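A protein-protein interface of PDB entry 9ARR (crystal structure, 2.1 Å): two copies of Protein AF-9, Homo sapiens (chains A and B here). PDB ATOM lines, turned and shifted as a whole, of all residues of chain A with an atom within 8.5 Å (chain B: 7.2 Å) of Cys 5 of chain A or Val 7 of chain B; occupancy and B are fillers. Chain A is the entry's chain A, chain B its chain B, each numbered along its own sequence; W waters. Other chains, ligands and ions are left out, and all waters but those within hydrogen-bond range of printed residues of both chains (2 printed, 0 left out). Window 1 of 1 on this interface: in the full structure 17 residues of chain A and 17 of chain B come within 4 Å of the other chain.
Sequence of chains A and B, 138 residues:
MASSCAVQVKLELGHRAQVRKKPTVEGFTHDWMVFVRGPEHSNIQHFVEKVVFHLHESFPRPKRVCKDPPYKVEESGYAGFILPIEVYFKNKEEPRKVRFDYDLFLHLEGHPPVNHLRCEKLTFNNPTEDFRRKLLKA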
ATOM      1  N   ALA A   2     -30.459  31.457 -12.696  1.00  0.00           N
ATOM      2  CA  ALA A   2     -29.107  30.932 -12.461  1.00  0.00           C
ATOM      3  C   ALA A   2     -28.654  30.041 -13.633  1.00  0.00           C
ATOM      4  O   ALA A   2     -27.492  30.051 -14.078  1.00  0.00           O
ATOM      5  CB  ALA A   2     -29.008  30.147 -11.171  1.00  0.00           C
ATOM      6  N   SER A   3     -29.600  29.257 -14.133  1.00  0.00           N
ATOM      7  CA  SER A   3     -29.310  28.250 -15.131  1.00  0.00           C
ATOM      8  C   SER A   3     -29.497  28.792 -16.542  1.00  0.00           C
ATOM      9  O   SER A   3     -30.271  29.715 -16.771  1.00  0.00           O
ATOM     10  CB  SER A   3     -30.167  27.054 -14.928  1.00  0.00           C
ATOM     11  OG  SER A   3     -31.479  27.373 -15.280  1.00  0.00           O
ATOM     12  N   SER A   4     -28.774  28.182 -17.477  1.00  0.00           N
ATOM     13  CA  SER A   4     -28.970  28.394 -18.901  1.00  0.00           C
ATOM     14  C   SER A   4     -28.594  27.096 -19.617  1.00  0.00           C
ATOM     15  O   SER A   4     -27.915  26.232 -19.052  1.00  0.00           O
ATOM     16  CB  SER A   4     -28.099  29.528 -19.357  1.00  0.00           C
ATOM     17  OG  SER A   4     -26.750  29.100 -19.219  1.00  0.00           O
ATOM     18  N   CYS A   5     -28.993  26.950 -20.879  1.00  0.00           N
ATOM     19  CA  CYS A   5     -28.559  25.790 -21.629  1.00  0.00           C
ATOM     20  C   CYS A   5     -28.427  26.084 -23.117  1.00  0.00           C
ATOM     21  O   CYS A   5     -28.983  27.025 -23.661  1.00  0.00           O
ATOM     22  CB  CYS A   5     -29.464  24.589 -21.402  1.00  0.00           C
ATOM     23  SG  CYS A   5     -31.071  24.778 -22.180  1.00  0.00           S
ATOM     24  N   ALA A   6     -27.602  25.252 -23.728  1.00  0.00           N
ATOM     25  CA  ALA A   6     -27.356  25.226 -25.158  1.00  0.00           C
ATOM     26  C   ALA A   6     -27.740  23.831 -25.616  1.00  0.00           C
ATOM     27  O   ALA A   6     -27.274  22.835 -25.041  1.00  0.00           O
ATOM     28  CB  ALA A   6     -25.901  25.573 -25.469  1.00  0.00           C
ATOM     29  N   VAL A   7     -28.661  23.759 -26.592  1.00  0.00           N
ATOM     30  CA  VAL A   7     -28.977  22.489 -27.218  1.00  0.00           C
ATOM     31  C   VAL A   7     -28.397  22.494 -28.626  1.00  0.00           C
ATOM     32  O   VAL A   7     -28.557  23.455 -29.375  1.00  0.00           O
ATOM     33  CB  VAL A   7     -30.474  22.175 -27.200  1.00  0.00           C
ATOM     34  CG1 VAL A   7     -30.763  20.867 -27.901  1.00  0.00           C
ATOM     35  CG2 VAL A   7     -31.002  22.141 -25.775  1.00  0.00           C
ATOM     36  N   GLN A   8     -27.655  21.429 -28.928  1.00  0.00           N
ATOM     37  CA  GLN A   8     -27.110  21.186 -30.252  1.00  0.00           C
ATOM     38  C   GLN A   8     -27.812  20.010 -30.929  1.00  0.00           C
ATOM     39  O   GLN A   8     -28.059  18.959 -30.289  1.00  0.00           O
ATOM     40  CB  GLN A   8     -25.637  20.821 -30.128  1.00  0.00           C
ATOM     41  CG  GLN A   8     -24.907  20.904 -31.440  1.00  0.00           C
ATOM     42  CD  GLN A   8     -23.466  21.211 -31.133  1.00  0.00           C
ATOM     43  OE1 GLN A   8     -23.176  22.133 -30.368  1.00  0.00           O
ATOM     44  NE2 GLN A   8     -22.574  20.415 -31.700  1.00  0.00           N
ATOM     45  N   THR A 123     -27.105  25.045 -33.150  1.00  0.00           N
ATOM     46  CA  THR A 123     -27.042  25.339 -31.725  1.00  0.00           C
ATOM     47  C   THR A 123     -28.222  26.224 -31.352  1.00  0.00           C
ATOM     48  O   THR A 123     -28.385  27.301 -31.915  1.00  0.00           O
ATOM     49  CB  THR A 123     -25.679  25.933 -31.346  1.00  0.00           C
ATOM     50  OG1 THR A 123     -24.748  24.905 -31.667  1.00  0.00           O
ATOM     51  CG2 THR A 123     -25.524  26.273 -29.876  1.00  0.00           C
ATOM     52  N   PHE A 124     -29.037  25.776 -30.398  1.00  0.00           N
ATOM     53  CA  PHE A 124     -30.083  26.650 -29.887  1.00  0.00           C
ATOM     54  C   PHE A 124     -29.781  27.027 -28.438  1.00  0.00           C
ATOM     55  O   PHE A 124     -29.674  26.136 -27.594  1.00  0.00           O
ATOM     56  CB  PHE A 124     -31.446  25.975 -29.947  1.00  0.00           C
ATOM     57  CG  PHE A 124     -31.862  25.555 -31.322  1.00  0.00           C
ATOM     58  CD1 PHE A 124     -31.445  24.330 -31.835  1.00  0.00           C
ATOM     59  CD2 PHE A 124     -32.648  26.394 -32.102  1.00  0.00           C
ATOM     60  CE1 PHE A 124     -31.824  23.941 -33.107  1.00  0.00           C
ATOM     61  CE2 PHE A 124     -33.031  25.995 -33.378  1.00  0.00           C
ATOM     62  CZ  PHE A 124     -32.608  24.781 -33.880  1.00  0.00           C
ATOM     63  N   ASN A 125     -29.649  28.332 -28.184  1.00  0.00           N
ATOM     64  CA  ASN A 125     -29.382  28.843 -26.845  1.00  0.00           C
ATOM     65  C   ASN A 125     -30.692  29.169 -26.137  1.00  0.00           C
ATOM     66  O   ASN A 125     -31.514  29.892 -26.668  1.00  0.00           O
ATOM     67  CB  ASN A 125     -28.455  30.050 -26.889  1.00  0.00           C
ATOM     68  CG  ASN A 125     -27.076  29.665 -27.381  1.00  0.00           C
ATOM     69  OD1 ASN A 125     -26.501  28.665 -26.966  1.00  0.00           O
ATOM     70  ND2 ASN A 125     -26.546  30.429 -28.305  1.00  0.00           N
ATOM     71  N   ASN A 126     -30.895  28.552 -24.972  1.00  0.00           N
ATOM     72  CA  ASN A 126     -32.043  28.802 -24.129  1.00  0.00           C
ATOM     73  C   ASN A 126     -33.317  28.704 -24.944  1.00  0.00           C
ATOM     74  O   ASN A 126     -34.104  29.629 -24.981  1.00  0.00           O
ATOM     75  CB  ASN A 126     -31.919  30.162 -23.452  1.00  0.00           C
ATOM     76  CG  ASN A 126     -30.718  30.158 -22.536  1.00  0.00           C
ATOM     77  OD1 ASN A 126     -30.618  29.310 -21.646  1.00  0.00           O
ATOM     78  ND2 ASN A 126     -29.776  31.051 -22.777  1.00  0.00           N
ATOM     79  N   PRO A 127     -33.567  27.571 -25.616  1.00  0.00           N
ATOM     80  CA  PRO A 127     -34.870  27.347 -26.228  1.00  0.00           C
ATOM     81  C   PRO A 127     -35.950  27.343 -25.147  1.00  0.00           C
ATOM     82  O   PRO A 127     -35.662  27.073 -23.989  1.00  0.00           O
ATOM     83  CB  PRO A 127     -34.744  25.959 -26.874  1.00  0.00           C
ATOM     84  CG  PRO A 127     -33.604  25.298 -26.108  1.00  0.00           C
ATOM     85  CD  PRO A 127     -32.660  26.430 -25.764  1.00  0.00           C
ATOM     86  N   THR A 128     -37.195  27.554 -25.565  1.00  0.00           N
ATOM     87  CA  THR A 128     -38.338  27.416 -24.688  1.00  0.00           C
ATOM     88  C   THR A 128     -38.379  25.984 -24.207  1.00  0.00           C
ATOM     89  O   THR A 128     -37.744  25.124 -24.804  1.00  0.00           O
ATOM     90  CB  THR A 128     -39.686  27.611 -25.395  1.00  0.00           C
ATOM     91  OG1 THR A 128     -39.818  26.571 -26.368  1.00  0.00           O
ATOM     92  CG2 THR A 128     -39.852  28.952 -26.069  1.00  0.00           C
ATOM     93  N   GLU A 129     -39.190  25.744 -23.182  1.00  0.00           N
ATOM     94  CA  GLU A 129     -39.319  24.423 -22.599  1.00  0.00           C
ATOM     95  C   GLU A 129     -39.856  23.468 -23.659  1.00  0.00           C
ATOM     96  O   GLU A 129     -39.338  22.363 -23.816  1.00  0.00           O
ATOM     97  CB  GLU A 129     -40.201  24.457 -21.350  1.00  0.00           C
ATOM     98  CG  GLU A 129     -40.419  23.094 -20.736  1.00  0.00           C
ATOM     99  CD  GLU A 129     -41.173  23.114 -19.419  1.00  0.00           C
ATOM    100  OE1 GLU A 129     -40.659  23.700 -18.457  1.00  0.00           O
ATOM    101  OE2 GLU A 129     -42.247  22.493 -19.347  1.00  0.00           O
ATOM    102  N   ARG A 132     -37.299  22.794 -26.287  1.00  0.00           N
ATOM    103  CA  ARG A 132     -36.143  22.127 -25.722  1.00  0.00           C
ATOM    104  C   ARG A 132     -36.466  20.645 -25.686  1.00  0.00           C
ATOM    105  O   ARG A 132     -35.614  19.824 -26.030  1.00  0.00           O
ATOM    106  CB  ARG A 132     -35.779  22.686 -24.335  1.00  0.00           C
ATOM    107  CG  ARG A 132     -34.517  22.080 -23.732  1.00  0.00           C
ATOM    108  CD  ARG A 132     -34.206  22.564 -22.327  1.00  0.00           C
ATOM    109  NE  ARG A 132     -35.294  22.202 -21.418  1.00  0.00           N
ATOM    110  CZ  ARG A 132     -36.042  23.084 -20.762  1.00  0.00           C
ATOM    111  NH1 ARG A 132     -35.825  24.370 -20.894  1.00  0.00           N
ATOM    112  NH2 ARG A 132     -37.022  22.677 -19.987  1.00  0.00           N
ATOM    113  N   LEU A 135     -36.364  19.155 -29.289  1.00  0.00           N
ATOM    114  CA  LEU A 135     -34.989  18.964 -29.704  1.00  0.00           C
ATOM    115  C   LEU A 135     -34.391  17.728 -29.032  1.00  0.00           C
ATOM    116  O   LEU A 135     -33.635  16.985 -29.645  1.00  0.00           O
ATOM    117  CB  LEU A 135     -34.149  20.200 -29.378  1.00  0.00           C
ATOM    118  CG  LEU A 135     -34.544  21.474 -30.107  1.00  0.00           C
ATOM    119  CD1 LEU A 135     -33.973  22.702 -29.416  1.00  0.00           C
ATOM    120  CD2 LEU A 135     -34.093  21.422 -31.563  1.00  0.00           C
ATOM    121  N   LEU A 136     -34.726  17.506 -27.765  1.00  0.00           N
ATOM    122  CA  LEU A 136     -33.990  16.523 -26.979  1.00  0.00           C
ATOM    123  C   LEU A 136     -34.652  15.161 -27.070  1.00  0.00           C
ATOM    124  O   LEU A 136     -34.069  14.177 -26.649  1.00  0.00           O
ATOM    125  CB  LEU A 136     -33.833  17.035 -25.546  1.00  0.00           C
ATOM    126  CG  LEU A 136     -32.757  18.118 -25.398  1.00  0.00           C
ATOM    127  CD1 LEU A 136     -32.757  18.728 -24.007  1.00  0.00           C
ATOM    128  CD2 LEU A 136     -31.388  17.538 -25.711  1.00  0.00           C
ATOM    129  N   CYS B   5     -26.994  18.520 -25.085  1.00  0.00           N
ATOM    130  CA  CYS B   5     -27.416  19.602 -24.206  1.00  0.00           C
ATOM    131  C   CYS B   5     -26.270  19.921 -23.254  1.00  0.00           C
ATOM    132  O   CYS B   5     -25.762  18.987 -22.634  1.00  0.00           O
ATOM    133  CB  CYS B   5     -28.589  19.131 -23.354  1.00  0.00           C
ATOM    134  SG  CYS B   5     -29.358  20.482 -22.430  1.00  0.00           S
ATOM    135  N   ALA B   6     -25.817  21.180 -23.180  1.00  0.00           N
ATOM    136  CA  ALA B   6     -24.980  21.610 -22.065  1.00  0.00           C
ATOM    137  C   ALA B   6     -25.804  22.555 -21.170  1.00  0.00           C
ATOM    138  O   ALA B   6     -26.358  23.537 -21.665  1.00  0.00           O
ATOM    139  CB  ALA B   6     -23.691  22.246 -22.569  1.00  0.00           C
ATOM    140  N   VAL B   7     -25.921  22.227 -19.880  1.00  0.00           N
ATOM    141  CA  VAL B   7     -26.551  23.118 -18.916  1.00  0.00           C
ATOM    142  C   VAL B   7     -25.476  23.763 -18.043  1.00  0.00           C
ATOM    143  O   VAL B   7     -24.604  23.076 -17.508  1.00  0.00           O
ATOM    144  CB  VAL B   7     -27.591  22.378 -18.065  1.00  0.00           C
ATOM    145  CG1 VAL B   7     -28.221  23.319 -17.055  1.00  0.00           C
ATOM    146  CG2 VAL B   7     -28.653  21.714 -18.924  1.00  0.00           C
ATOM    147  N   GLN B   8     -25.529  25.096 -17.982  1.00  0.00           N
ATOM    148  CA  GLN B   8     -24.676  25.913 -17.124  1.00  0.00           C
ATOM    149  C   GLN B   8     -25.475  26.467 -15.946  1.00  0.00           C
ATOM    150  O   GLN B   8     -26.633  26.852 -16.125  1.00  0.00           O
ATOM    151  CB  GLN B   8     -24.095  27.107 -17.855  1.00  0.00           C
ATOM    152  CG  GLN B   8     -23.122  26.717 -18.944  1.00  0.00           C
ATOM    153  CD  GLN B   8     -22.275  27.911 -19.292  1.00  0.00           C
ATOM    154  OE1 GLN B   8     -22.207  28.889 -18.547  1.00  0.00           O
ATOM    155  NE2 GLN B   8     -21.597  27.826 -20.422  1.00  0.00           N
ATOM    156  N   VAL B   9     -24.852  26.503 -14.752  1.00  0.00           N
ATOM    157  CA  VAL B   9     -25.463  27.138 -13.603  1.00  0.00           C
ATOM    158  C   VAL B   9     -24.398  27.963 -12.931  1.00  0.00           C
ATOM    159  O   VAL B   9     -23.244  27.541 -12.787  1.00  0.00           O
ATOM    160  CB  VAL B   9     -26.148  26.202 -12.584  1.00  0.00           C
ATOM    161  CG1 VAL B   9     -27.424  25.579 -13.114  1.00  0.00           C
ATOM    162  CG2 VAL B   9     -25.231  25.104 -12.120  1.00  0.00           C
ATOM    163  N   LEU B 122     -20.936  26.183 -13.077  1.00  0.00           N
ATOM    164  CA  LEU B 122     -20.912  24.759 -13.329  1.00  0.00           C
ATOM    165  C   LEU B 122     -21.452  24.468 -14.728  1.00  0.00           C
ATOM    166  O   LEU B 122     -22.413  25.109 -15.159  1.00  0.00           O
ATOM    167  CB  LEU B 122     -21.838  24.123 -12.308  1.00  0.00           C
ATOM    168  CG  LEU B 122     -21.510  24.447 -10.856  1.00  0.00           C
ATOM    169  CD1 LEU B 122     -22.472  23.721  -9.939  1.00  0.00           C
ATOM    170  CD2 LEU B 122     -20.084  24.067 -10.530  1.00  0.00           C
ATOM    171  N   THR B 123     -20.871  23.460 -15.383  1.00  0.00           N
ATOM    172  CA  THR B 123     -21.334  22.980 -16.675  1.00  0.00           C
ATOM    173  C   THR B 123     -21.719  21.517 -16.538  1.00  0.00           C
ATOM    174  O   THR B 123     -20.915  20.713 -16.113  1.00  0.00           O
ATOM    175  CB  THR B 123     -20.277  23.226 -17.749  1.00  0.00           C
ATOM    176  OG1 THR B 123     -19.967  24.630 -17.684  1.00  0.00           O
ATOM    177  CG2 THR B 123     -20.766  22.862 -19.142  1.00  0.00           C
ATOM    178  N   PHE B 124     -22.968  21.167 -16.859  1.00  0.00           N
ATOM    179  CA  PHE B 124     -23.324  19.762 -16.920  1.00  0.00           C
ATOM    180  C   PHE B 124     -23.619  19.377 -18.365  1.00  0.00           C
ATOM    181  O   PHE B 124     -24.481  19.992 -19.002  1.00  0.00           O
ATOM    182  CB  PHE B 124     -24.532  19.472 -16.062  1.00  0.00           C
ATOM    183  CG  PHE B 124     -24.358  19.839 -14.621  1.00  0.00           C
ATOM    184  CD1 PHE B 124     -24.604  21.131 -14.190  1.00  0.00           C
ATOM    185  CD2 PHE B 124     -23.907  18.900 -13.709  1.00  0.00           C
ATOM    186  CE1 PHE B 124     -24.429  21.483 -12.858  1.00  0.00           C
ATOM    187  CE2 PHE B 124     -23.745  19.251 -12.376  1.00  0.00           C
ATOM    188  CZ  PHE B 124     -24.003  20.546 -11.957  1.00  0.00           C
ATOM    189  N   ASN B 125     -22.876  18.382 -18.881  1.00  0.00           N
ATOM    190  CA  ASN B 125     -23.044  17.914 -20.258  1.00  0.00           C
ATOM    191  C   ASN B 125     -23.994  16.724 -20.276  1.00  0.00           C
ATOM    192  O   ASN B 125     -23.795  15.758 -19.563  1.00  0.00           O
ATOM    193  CB  ASN B 125     -21.704  17.591 -20.904  1.00  0.00           C
ATOM    194  CG  ASN B 125     -20.882  18.855 -21.084  1.00  0.00           C
ATOM    195  OD1 ASN B 125     -21.373  19.876 -21.553  1.00  0.00           O
ATOM    196  ND2 ASN B 125     -19.632  18.831 -20.670  1.00  0.00           N
ATOM    197  N   ASN B 126     -25.072  16.854 -21.029  1.00  0.00           N
ATOM    198  CA  ASN B 126     -26.061  15.805 -21.199  1.00  0.00           C
ATOM    199  C   ASN B 126     -26.476  15.222 -19.876  1.00  0.00           C
ATOM    200  O   ASN B 126     -26.368  14.028 -19.678  1.00  0.00           O
ATOM    201  CB  ASN B 126     -25.524  14.720 -22.124  1.00  0.00           C
ATOM    202  CG  ASN B 126     -25.158  15.352 -23.442  1.00  0.00           C
ATOM    203  OD1 ASN B 126     -26.029  15.897 -24.124  1.00  0.00           O
ATOM    204  ND2 ASN B 126     -23.870  15.386 -23.727  1.00  0.00           N
ATOM    205  N   PRO B 127     -26.990  16.031 -18.939  1.00  0.00           N
ATOM    206  CA  PRO B 127     -27.552  15.465 -17.717  1.00  0.00           C
ATOM    207  C   PRO B 127     -28.740  14.589 -18.074  1.00  0.00           C
ATOM    208  O   PRO B 127     -29.330  14.790 -19.112  1.00  0.00           O
ATOM    209  CB  PRO B 127     -28.015  16.703 -16.920  1.00  0.00           C
ATOM    210  CG  PRO B 127     -28.091  17.824 -17.951  1.00  0.00           C
ATOM    211  CD  PRO B 127     -27.028  17.506 -18.982  1.00  0.00           C
ATOM    212  N   PHE B 131     -32.584  15.457 -13.843  1.00  0.00           N
ATOM    213  CA  PHE B 131     -31.634  16.429 -13.372  1.00  0.00           C
ATOM    214  C   PHE B 131     -31.698  17.684 -14.227  1.00  0.00           C
ATOM    215  O   PHE B 131     -31.621  18.796 -13.698  1.00  0.00           O
ATOM    216  CB  PHE B 131     -30.233  15.809 -13.351  1.00  0.00           C
ATOM    217  CG  PHE B 131     -29.233  16.655 -12.612  1.00  0.00           C
ATOM    218  CD1 PHE B 131     -29.583  17.286 -11.422  1.00  0.00           C
ATOM    219  CD2 PHE B 131     -27.947  16.828 -13.110  1.00  0.00           C
ATOM    220  CE1 PHE B 131     -28.667  18.105 -10.783  1.00  0.00           C
ATOM    221  CE2 PHE B 131     -27.021  17.597 -12.432  1.00  0.00           C
ATOM    222  CZ  PHE B 131     -27.389  18.251 -11.286  1.00  0.00           C
ATOM    223  N   ARG B 132     -31.840  17.490 -15.545  1.00  0.00           N
ATOM    224  CA  ARG B 132     -31.840  18.598 -16.477  1.00  0.00           C
ATOM    225  C   ARG B 132     -32.989  19.512 -16.080  1.00  0.00           C
ATOM    226  O   ARG B 132     -32.839  20.739 -16.066  1.00  0.00           O
ATOM    227  CB  ARG B 132     -31.961  18.133 -17.940  1.00  0.00           C
ATOM    228  CG  ARG B 132     -31.915  19.266 -18.968  1.00  0.00           C
ATOM    229  CD  ARG B 132     -32.134  18.841 -20.422  1.00  0.00           C
ATOM    230  NE  ARG B 132     -33.368  18.098 -20.623  1.00  0.00           N
ATOM    231  CZ  ARG B 132     -33.441  16.817 -20.961  1.00  0.00           C
ATOM    232  NH1 ARG B 132     -32.361  16.074 -21.100  1.00  0.00           N
ATOM    233  NH2 ARG B 132     -34.616  16.268 -21.144  1.00  0.00           N
ATOM    234  N   ARG B 133     -34.116  18.907 -15.697  1.00  0.00           N
ATOM    235  CA  ARG B 133     -35.282  19.714 -15.358  1.00  0.00           C
ATOM    236  C   ARG B 133     -35.046  20.452 -14.045  1.00  0.00           C
ATOM    237  O   ARG B 133     -35.490  21.592 -13.879  1.00  0.00           O
ATOM    238  CB  ARG B 133     -36.546  18.853 -15.329  1.00  0.00           C
ATOM    239  CG  ARG B 133     -36.954  18.445 -16.734  1.00  0.00           C
ATOM    240  CD  ARG B 133     -38.110  17.472 -16.773  1.00  0.00           C
ATOM    241  NE  ARG B 133     -38.218  16.910 -18.110  1.00  0.00           N
ATOM    242  CZ  ARG B 133     -39.345  16.533 -18.701  1.00  0.00           C
ATOM    243  NH1 ARG B 133     -40.503  16.773 -18.120  1.00  0.00           N
ATOM    244  NH2 ARG B 133     -39.306  15.896 -19.863  1.00  0.00           N
ATOM    245  N   LEU B 135     -32.105  21.427 -12.845  1.00  0.00           N
ATOM    246  CA  LEU B 135     -31.164  22.504 -13.072  1.00  0.00           C
ATOM    247  C   LEU B 135     -31.917  23.688 -13.647  1.00  0.00           C
ATOM    248  O   LEU B 135     -31.585  24.860 -13.358  1.00  0.00           O
ATOM    249  CB  LEU B 135     -30.055  22.040 -14.023  1.00  0.00           C
ATOM    250  CG  LEU B 135     -29.123  20.960 -13.461  1.00  0.00           C
ATOM    251  CD1 LEU B 135     -28.327  20.281 -14.554  1.00  0.00           C
ATOM    252  CD2 LEU B 135     -28.157  21.532 -12.435  1.00  0.00           C
ATOM    253  N   LEU B 136     -32.882  23.383 -14.536  1.00  0.00           N
ATOM    254  CA  LEU B 136     -33.407  24.441 -15.376  1.00  0.00           C
ATOM    255  C   LEU B 136     -34.594  25.113 -14.688  1.00  0.00           C
ATOM    256  O   LEU B 136     -34.990  26.189 -15.102  1.00  0.00           O
ATOM    257  CB  LEU B 136     -33.693  23.878 -16.765  1.00  0.00           C
ATOM    258  CG  LEU B 136     -32.436  23.721 -17.630  1.00  0.00           C
ATOM    259  CD1 LEU B 136     -32.733  23.023 -18.949  1.00  0.00           C
ATOM    260  CD2 LEU B 136     -31.783  25.077 -17.905  1.00  0.00           C
HETATM  261  O   HOH W   1     -26.315  29.886 -16.409  1.00  0.00           O
HETATM  262  O   HOH W   2     -36.549  19.513 -20.314  1.00  0.00           O
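Of the 16 printed residues of chain B, 8 touch a printed residue of chain A. Hydrophobic or aromatic side chains of chain B within 4 Å of the printed part of chain A: Val 7, Val 9 and Leu 136. Of the 17 printed residues of chain A, 7 touch a printed residue of chain B. Printed residues of chain A that touch a printed residue of chain B: Ala 2, Ser 3, Ser 4, Cys 5, Ala 6, Arg 132 and Leu 136. Hydrophobic or aromatic side chains of chain A within 4 Å of the printed part of chain B: Leu 136. Among the printed residues, 15 pairs touch across the chains. Among the printed residues, no Asp or Glu carboxylate lies within 4 Å of a Lys or Arg side-chain nitrogen of the other chain.
Water W1 lies within hydrogen-bond range of the backbone carbonyl oxygen (O) of Ala 2 of chain A, the side-chain hydroxyl (OG) of Ser 4 of chain A and the backbone carbonyl oxygen (O) of Gln 8 of chain B. Water W2 bridges the guanidinium group (NE) of Arg 132 of chain A (3.2 Å) and the guanidinium group (NE) of Arg 132 of chain B (3.5 Å).
Cys 5 of chain A touches Ala 6 of chain B, and with the chains exchanged Ala 6 of chain A touches Cys 5 of chain B. Cys 5 of chain A touches Val 7 of chain B, but with the chains exchanged Val 7 of chain A does not touch Cys 5 of chain B (4.1 Å). Arg 132 of chain A touches Leu 136 of chain B, and with the chains exchanged Leu 136 of chain A touches Arg 132 of chain B. Leu 136 of chain A touches Cys 5 of chain B, but with the chains exchanged Cys 5 of chain A does not touch Leu 136 of chain B (4.04 Å). Positions printed for both chains: 5, 6, 7, 8, 123, 124, 125, 126, 127, 132, 135 and 136.
Val 7 of chain B touches just these residues of chain A: Ser 4 and Cys 5. Of the printed residues of chain A, Ala 6 of chain B touches Cys 5 (3.1 Å) and Ala 6 (2.9 Å). Of the printed residues of chain A, Leu 135 of chain B touches Ser 3 (3.0 Å). Of the printed residues of chain A, Val 9 of chain B touches Ala 2 (3.6 Å) and Ser 3 (3.6 Å). Of the printed residues of chain A, Leu 136 of chain B touches Ser 3 and Arg 132. Printed residues of chain B within 4 Å of Ala 6 of chain A: Cys 5 (3.3 Å) and Ala 6 (2.9 Å). Phe 124 of chain A touches none of the printed residues of chain B. Glu 129 of chain A touches none of the printed residues of chain B. The nearest residue of chain B that does not touch Cys 5 of chain A is Leu 136 of chain B (4.04 Å). The nearest printed residue of chain A that does not touch Leu 135 of chain B is Ala 2 of chain A (6.0 Å).
N of Gln 8 of chain B sits at hydrogen-bond distance from O of Ser 4 of chain A, 2.9 Å away. The backbone carbonyl oxygen (O) of Ala 6 of chain A is in hydrogen-bond range of the backbone NH (N) of Ala 6 of chain B (2.9 Å). O of Leu 135 of chain B sits close to OG of Ser 3 of chain A, at 3.2 Å.
Among the printed residues, pairs that only touch across the chains: Ala 2 of chain A with Gln 8 of chain B, Ala 2 of chain A with Val 9 of chain B, Ser 3 of chain A with Gln 8 of chain B, Ser 3 of chain A with Val 9 of chain B, Ser 3 of chain A with Leu 136 of chain B, Ser 4 of chain A with Val 7 of chain B, Cys 5 of chain A with Ala 6 of chain B, Cys 5 of chain A with Val 7 of chain B, Ala 6 of chain A with Cys 5 of chain B, Arg 132 of chain A with Leu 136 of chain B, Leu 136 of chain A with Cys 5 of chain B and Leu 136 of chain A with Arg 132 of chain B.
The backbone carbonyl oxygen (O) of Val 7 of chain B sits at hydrogen-bond distance from the backbone NH (N) of Phe 124 of chain B (2.6 Å). The backbone NH (N) of Leu 122 of chain B sits at hydrogen-bond distance from the backbone carbonyl oxygen (O) of Val 9 of chain B. The backbone carbonyl oxygen (O) of Cys 5 of chain B is in hydrogen-bond range of the backbone NH (N) of Asn 126 of chain B (2.8 Å). O of Cys 5 of chain A lies within hydrogen-bond range of N of Asn 126 of chain A (2.8 Å).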
